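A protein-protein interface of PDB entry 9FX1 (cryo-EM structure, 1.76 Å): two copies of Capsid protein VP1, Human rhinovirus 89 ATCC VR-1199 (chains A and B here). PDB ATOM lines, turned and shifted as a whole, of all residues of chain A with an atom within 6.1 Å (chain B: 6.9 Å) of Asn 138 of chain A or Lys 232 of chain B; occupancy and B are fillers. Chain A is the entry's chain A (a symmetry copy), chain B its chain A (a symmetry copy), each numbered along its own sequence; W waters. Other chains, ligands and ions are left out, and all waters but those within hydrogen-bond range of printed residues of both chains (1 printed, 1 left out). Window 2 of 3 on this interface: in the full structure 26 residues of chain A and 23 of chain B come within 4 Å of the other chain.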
ATOM      1  N   ALA A 135     -15.208 -18.042   7.313  1.00  0.00           N
ATOM      2  CA  ALA A 135     -16.441 -17.877   6.553  1.00  0.00           C
ATOM      3  C   ALA A 135     -16.504 -18.889   5.393  1.00  0.00           C
ATOM      4  O   ALA A 135     -15.635 -18.890   4.521  1.00  0.00           O
ATOM      5  CB  ALA A 135     -16.509 -16.424   6.057  1.00  0.00           C
ATOM      6  N   GLN A 136     -17.517 -19.760   5.388  1.00  0.00           N
ATOM      7  CA  GLN A 136     -17.764 -20.730   4.311  1.00  0.00           C
ATOM      8  C   GLN A 136     -18.732 -20.209   3.232  1.00  0.00           C
ATOM      9  O   GLN A 136     -18.853 -20.816   2.169  1.00  0.00           O
ATOM     10  CB  GLN A 136     -18.283 -22.053   4.902  1.00  0.00           C
ATOM     11  CG  GLN A 136     -17.328 -22.669   5.935  1.00  0.00           C
ATOM     12  CD  GLN A 136     -15.906 -22.777   5.397  1.00  0.00           C
ATOM     13  OE1 GLN A 136     -15.620 -23.519   4.468  1.00  0.00           O
ATOM     14  NE2 GLN A 136     -14.968 -22.032   5.940  1.00  0.00           N
ATOM     15  N   GLY A 137     -19.425 -19.102   3.501  1.00  0.00           N
ATOM     16  CA  GLY A 137     -20.323 -18.430   2.565  1.00  0.00           C
ATOM     17  C   GLY A 137     -19.902 -16.983   2.284  1.00  0.00           C
ATOM     18  O   GLY A 137     -18.758 -16.590   2.510  1.00  0.00           O
ATOM     19  N   ASN A 138     -20.835 -16.181   1.774  1.00  0.00           N
ATOM     20  CA  ASN A 138     -20.559 -14.810   1.321  1.00  0.00           C
ATOM     21  C   ASN A 138     -20.468 -13.759   2.444  1.00  0.00           C
ATOM     22  O   ASN A 138     -20.093 -12.617   2.184  1.00  0.00           O
ATOM     23  CB  ASN A 138     -21.614 -14.422   0.271  1.00  0.00           C
ATOM     24  CG  ASN A 138     -21.514 -15.259  -0.992  1.00  0.00           C
ATOM     25  OD1 ASN A 138     -20.443 -15.663  -1.417  1.00  0.00           O
ATOM     26  ND2 ASN A 138     -22.617 -15.548  -1.641  1.00  0.00           N
ATOM     27  N   ASP A 139     -20.815 -14.111   3.681  1.00  0.00           N
ATOM     28  CA  ASP A 139     -20.768 -13.210   4.835  1.00  0.00           C
ATOM     29  C   ASP A 139     -20.491 -13.977   6.139  1.00  0.00           C
ATOM     30  O   ASP A 139     -20.842 -15.155   6.279  1.00  0.00           O
ATOM     31  CB  ASP A 139     -22.091 -12.430   4.904  1.00  0.00           C
ATOM     32  CG  ASP A 139     -22.135 -11.450   6.077  1.00  0.00           C
ATOM     33  OD1 ASP A 139     -21.158 -10.699   6.272  1.00  0.00           O
ATOM     34  OD2 ASP A 139     -23.121 -11.499   6.842  1.00  0.00           O
ATOM     35  N   SER A 140     -19.894 -13.310   7.125  1.00  0.00           N
ATOM     36  CA  SER A 140     -19.634 -13.875   8.457  1.00  0.00           C
ATOM     37  C   SER A 140     -20.905 -13.978   9.310  1.00  0.00           C
ATOM     38  O   SER A 140     -20.986 -14.833  10.193  1.00  0.00           O
ATOM     39  CB  SER A 140     -18.615 -13.003   9.202  1.00  0.00           C
ATOM     40  OG  SER A 140     -17.424 -12.850   8.443  1.00  0.00           O
ATOM     41  N   HIS A 233     -25.111 -18.243   6.422  1.00  0.00           N
ATOM     42  CA  HIS A 233     -23.779 -18.665   5.974  1.00  0.00           C
ATOM     43  C   HIS A 233     -22.947 -19.324   7.081  1.00  0.00           C
ATOM     44  O   HIS A 233     -22.642 -18.705   8.101  1.00  0.00           O
ATOM     45  CB  HIS A 233     -23.052 -17.461   5.373  1.00  0.00           C
ATOM     46  CG  HIS A 233     -23.732 -16.917   4.143  1.00  0.00           C
ATOM     47  ND1 HIS A 233     -23.788 -17.566   2.910  1.00  0.00           N
ATOM     48  CD2 HIS A 233     -24.386 -15.724   4.042  1.00  0.00           C
ATOM     49  CE1 HIS A 233     -24.479 -16.755   2.095  1.00  0.00           C
ATOM     50  NE2 HIS A 233     -24.846 -15.639   2.746  1.00  0.00           N
ATOM     51  N   SER B  85      -6.065 -19.571   0.151  1.00  0.00           N
ATOM     52  CA  SER B  85      -6.822 -20.430  -0.767  1.00  0.00           C
ATOM     53  C   SER B  85      -8.089 -20.981  -0.119  1.00  0.00           C
ATOM     54  O   SER B  85      -8.105 -21.294   1.073  1.00  0.00           O
ATOM     55  CB  SER B  85      -5.937 -21.565  -1.288  1.00  0.00           C
ATOM     56  OG  SER B  85      -6.623 -22.295  -2.285  1.00  0.00           O
ATOM     57  N   SER B  86      -9.150 -21.141  -0.907  1.00  0.00           N
ATOM     58  CA  SER B  86     -10.363 -21.853  -0.496  1.00  0.00           C
ATOM     59  C   SER B  86     -10.159 -23.372  -0.438  1.00  0.00           C
ATOM     60  O   SER B  86     -10.891 -24.051   0.280  1.00  0.00           O
ATOM     61  CB  SER B  86     -11.510 -21.503  -1.446  1.00  0.00           C
ATOM     62  OG  SER B  86     -11.189 -21.872  -2.776  1.00  0.00           O
ATOM     63  N   GLY B 137     -12.386 -11.827  -3.623  1.00  0.00           N
ATOM     64  CA  GLY B 137     -13.790 -12.195  -3.791  1.00  0.00           C
ATOM     65  C   GLY B 137     -14.743 -11.163  -3.178  1.00  0.00           C
ATOM     66  O   GLY B 137     -14.380 -10.013  -2.937  1.00  0.00           O
ATOM     67  N   ASN B 138     -15.986 -11.575  -2.931  1.00  0.00           N
ATOM     68  CA  ASN B 138     -17.058 -10.678  -2.477  1.00  0.00           C
ATOM     69  C   ASN B 138     -17.023 -10.332  -0.976  1.00  0.00           C
ATOM     70  O   ASN B 138     -17.782  -9.474  -0.528  1.00  0.00           O
ATOM     71  CB  ASN B 138     -18.410 -11.287  -2.885  1.00  0.00           C
ATOM     72  CG  ASN B 138     -18.591 -11.349  -4.391  1.00  0.00           C
ATOM     73  OD1 ASN B 138     -18.129 -10.496  -5.133  1.00  0.00           O
ATOM     74  ND2 ASN B 138     -19.268 -12.351  -4.899  1.00  0.00           N
ATOM     75  N   ASP B 139     -16.175 -10.988  -0.186  1.00  0.00           N
ATOM     76  CA  ASP B 139     -16.042 -10.750   1.254  1.00  0.00           C
ATOM     77  C   ASP B 139     -14.611 -11.036   1.743  1.00  0.00           C
ATOM     78  O   ASP B 139     -13.894 -11.868   1.177  1.00  0.00           O
ATOM     79  CB  ASP B 139     -17.079 -11.612   1.993  1.00  0.00           C
ATOM     80  CG  ASP B 139     -17.024 -11.425   3.509  1.00  0.00           C
ATOM     81  OD1 ASP B 139     -16.987 -10.268   3.973  1.00  0.00           O
ATOM     82  OD2 ASP B 139     -16.939 -12.449   4.221  1.00  0.00           O
ATOM     83  N   SER B 140     -14.193 -10.380   2.822  1.00  0.00           N
ATOM     84  CA  SER B 140     -12.887 -10.599   3.460  1.00  0.00           C
ATOM     85  C   SER B 140     -12.833 -11.914   4.251  1.00  0.00           C
ATOM     86  O   SER B 140     -11.756 -12.488   4.417  1.00  0.00           O
ATOM     87  CB  SER B 140     -12.574  -9.440   4.417  1.00  0.00           C
ATOM     88  OG  SER B 140     -12.637  -8.192   3.743  1.00  0.00           O
ATOM     89  N   GLY B 141     -13.970 -12.413   4.743  1.00  0.00           N
ATOM     90  CA  GLY B 141     -14.009 -13.458   5.766  1.00  0.00           C
ATOM     91  C   GLY B 141     -13.488 -12.948   7.116  1.00  0.00           C
ATOM     92  O   GLY B 141     -13.361 -11.740   7.333  1.00  0.00           O
ATOM     93  N   SER B 229      -8.811 -21.092   9.267  1.00  0.00           N
ATOM     94  CA  SER B 229      -8.821 -22.195   8.299  1.00  0.00           C
ATOM     95  C   SER B 229      -9.326 -21.727   6.921  1.00  0.00           C
ATOM     96  O   SER B 229      -9.613 -20.547   6.718  1.00  0.00           O
ATOM     97  CB  SER B 229      -9.623 -23.374   8.872  1.00  0.00           C
ATOM     98  OG  SER B 229     -10.939 -23.015   9.241  1.00  0.00           O
ATOM     99  N   ASN B 230      -9.351 -22.600   5.912  1.00  0.00           N
ATOM    100  CA  ASN B 230      -9.708 -22.208   4.546  1.00  0.00           C
ATOM    101  C   ASN B 230     -11.113 -21.576   4.483  1.00  0.00           C
ATOM    102  O   ASN B 230     -12.057 -22.067   5.093  1.00  0.00           O
ATOM    103  CB  ASN B 230      -9.574 -23.399   3.580  1.00  0.00           C
ATOM    104  CG  ASN B 230     -10.497 -24.560   3.901  1.00  0.00           C
ATOM    105  OD1 ASN B 230     -10.394 -25.186   4.944  1.00  0.00           O
ATOM    106  ND2 ASN B 230     -11.394 -24.912   3.010  1.00  0.00           N
ATOM    107  N   GLN B 231     -11.245 -20.495   3.714  1.00  0.00           N
ATOM    108  CA  GLN B 231     -12.468 -19.699   3.579  1.00  0.00           C
ATOM    109  C   GLN B 231     -12.860 -19.554   2.107  1.00  0.00           C
ATOM    110  O   GLN B 231     -12.020 -19.693   1.221  1.00  0.00           O
ATOM    111  CB  GLN B 231     -12.272 -18.309   4.204  1.00  0.00           C
ATOM    112  CG  GLN B 231     -12.071 -18.358   5.716  1.00  0.00           C
ATOM    113  CD  GLN B 231     -11.899 -16.970   6.310  1.00  0.00           C
ATOM    114  OE1 GLN B 231     -12.851 -16.362   6.766  1.00  0.00           O
ATOM    115  NE2 GLN B 231     -10.699 -16.430   6.332  1.00  0.00           N
ATOM    116  N   LYS B 232     -14.128 -19.240   1.832  1.00  0.00           N
ATOM    117  CA  LYS B 232     -14.659 -19.175   0.464  1.00  0.00           C
ATOM    118  C   LYS B 232     -13.910 -18.200  -0.453  1.00  0.00           C
ATOM    119  O   LYS B 232     -13.632 -18.546  -1.597  1.00  0.00           O
ATOM    120  CB  LYS B 232     -16.154 -18.828   0.540  1.00  0.00           C
ATOM    121  CG  LYS B 232     -16.822 -18.905  -0.839  1.00  0.00           C
ATOM    122  CD  LYS B 232     -18.323 -18.643  -0.731  1.00  0.00           C
ATOM    123  CE  LYS B 232     -18.945 -18.658  -2.130  1.00  0.00           C
ATOM    124  NZ  LYS B 232     -20.391 -18.335  -2.088  1.00  0.00           N
ATOM    125  N   HIS B 233     -13.570 -17.004   0.038  1.00  0.00           N
ATOM    126  CA  HIS B 233     -13.000 -15.923  -0.775  1.00  0.00           C
ATOM    127  C   HIS B 233     -11.528 -15.636  -0.457  1.00  0.00           C
ATOM    128  O   HIS B 233     -11.179 -15.266   0.666  1.00  0.00           O
ATOM    129  CB  HIS B 233     -13.860 -14.670  -0.606  1.00  0.00           C
ATOM    130  CG  HIS B 233     -15.268 -14.849  -1.113  1.00  0.00           C
ATOM    131  ND1 HIS B 233     -15.621 -14.976  -2.456  1.00  0.00           N
ATOM    132  CD2 HIS B 233     -16.400 -14.912  -0.353  1.00  0.00           C
ATOM    133  CE1 HIS B 233     -16.955 -15.121  -2.477  1.00  0.00           C
ATOM    134  NE2 HIS B 233     -17.449 -15.081  -1.229  1.00  0.00           N
ATOM    135  N   ASP B 234     -10.667 -15.732  -1.465  1.00  0.00           N
ATOM    136  CA  ASP B 234      -9.220 -15.574  -1.313  1.00  0.00           C
ATOM    137  C   ASP B 234      -8.808 -14.145  -0.938  1.00  0.00           C
ATOM    138  O   ASP B 234      -9.502 -13.171  -1.230  1.00  0.00           O
ATOM    139  CB  ASP B 234      -8.489 -16.042  -2.582  1.00  0.00           C
ATOM    140  CG  ASP B 234      -8.642 -17.548  -2.864  1.00  0.00           C
ATOM    141  OD1 ASP B 234      -9.150 -18.291  -1.995  1.00  0.00           O
ATOM    142  OD2 ASP B 234      -8.234 -17.980  -3.966  1.00  0.00           O
HETATM  143  O   HOH W   1     -16.830 -14.916   3.395  1.00  0.00           O
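The backbone carbonyl oxygen of Asn 230 of chain B lies within hydrogen-bond range of the side-chain amide nitrogen of Gln 136 of chain A (3.0 Å).
The backbone NH of Ala 135 of chain A sits at hydrogen-bond distance from the side-chain amide oxygen of Gln 231 of chain B, at 2.9 Å.
The backbone carbonyl oxygen (O) of Ala 135 of chain A lies within hydrogen-bond range of the backbone NH (N) of Lys 232 of chain B (3.1 Å).
NZ of Lys 232 of chain B is in hydrogen-bond range of OD1 of Asn 138 of chain A, at 2.8 Å.
A ring nitrogen (NE2) of His 233 of chain B sits at hydrogen-bond distance from the side-chain amide oxygen (OD1) of Asn 138 of chain A (3.1 Å).
The side-chain amide nitrogen of Asn 230 of chain B is in hydrogen-bond range of the backbone carbonyl oxygen of Ser 86 of chain B, at 2.9 Å.
The backbone NH of Asn 138 of chain B sits at hydrogen-bond distance from a ring nitrogen (ND1) of His 233 of chain B, at 3.5 Å.
The backbone NH of Gly 141 of chain B sits at hydrogen-bond distance from the side-chain carboxylate of Asp 139 of chain B (3.0 Å).
The backbone NH of Asn 138 of chain A lies within hydrogen-bond range of a ring nitrogen (ND1) of His 233 of chain A (3.5 Å).
Among the printed residues, pairs that only touch across the chains: Ala 135 of chain A with Gly 141 of chain B (3.9 Å), Gln 136 of chain A with Lys 232 of chain B (3.7 Å), Gly 137 of chain A with Lys 232 of chain B (3.8 Å), Asn 138 of chain A with Asp 139 of chain B (3.2 Å) and Asp 139 of chain A with Asp 139 of chain B (3.95 Å).
Printed residues of chain B within 4 Å of Gln 136 of chain A: Asn 230 and Lys 232.
Of chain B, only Asp 139, Lys 232 and His 233 come within 4 Å of Asn 138 of chain A.
Of the printed residues of chain B, Asp 139 of chain A touches Asp 139 (3.95 Å).
Ser 85 of chain B touches none of the printed residues of chain A.
Of the printed residues of chain A, Asn 230 of chain B touches Gln 136.
The nearest residue of chain B that does not touch Asn 138 of chain A is Asn 138 of chain B (4.8 Å).
The nearest printed residue of chain B that does not touch Gln 136 of chain A is Gln 231 of chain B (4.2 Å).
Printed residues of chain A that touch a printed residue of chain B: Ala 135, Gln 136, Gly 137, Asn 138 and Asp 139.
Hydrophobic or aromatic side chains of chain A that line the printed part of chain B: Ala 135.
Printed residues of chain B that touch a printed residue of chain A: Asp 139, Gly 141, Asn 230, Gln 231, Lys 232 and His 233.
Hydrophobic or aromatic side chains of chain B that line the printed part of chain A: His 233.
Asn 138 of chain A touches Asp 139 of chain B, but with the chains exchanged Asp 139 of chain A does not touch Asn 138 of chain B (7.0 Å).
Asn 138 of chain A touches His 233 of chain B, but with the chains exchanged His 233 of chain A does not touch Asn 138 of chain B (9.6 Å).
Asp 139 of chain B touches its own counterpart, Asp 139 of chain A.
Positions printed for both chains: 137, 138, 139, 140 and 233.
Of the 10 pairs that touch across the chains among the printed residues, 1 has its exchanged pair printed and touching as well.
Water W1 lies within hydrogen-bond range of OD2 of Asp 139 of chain B and O of Gly 137 of chain A.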
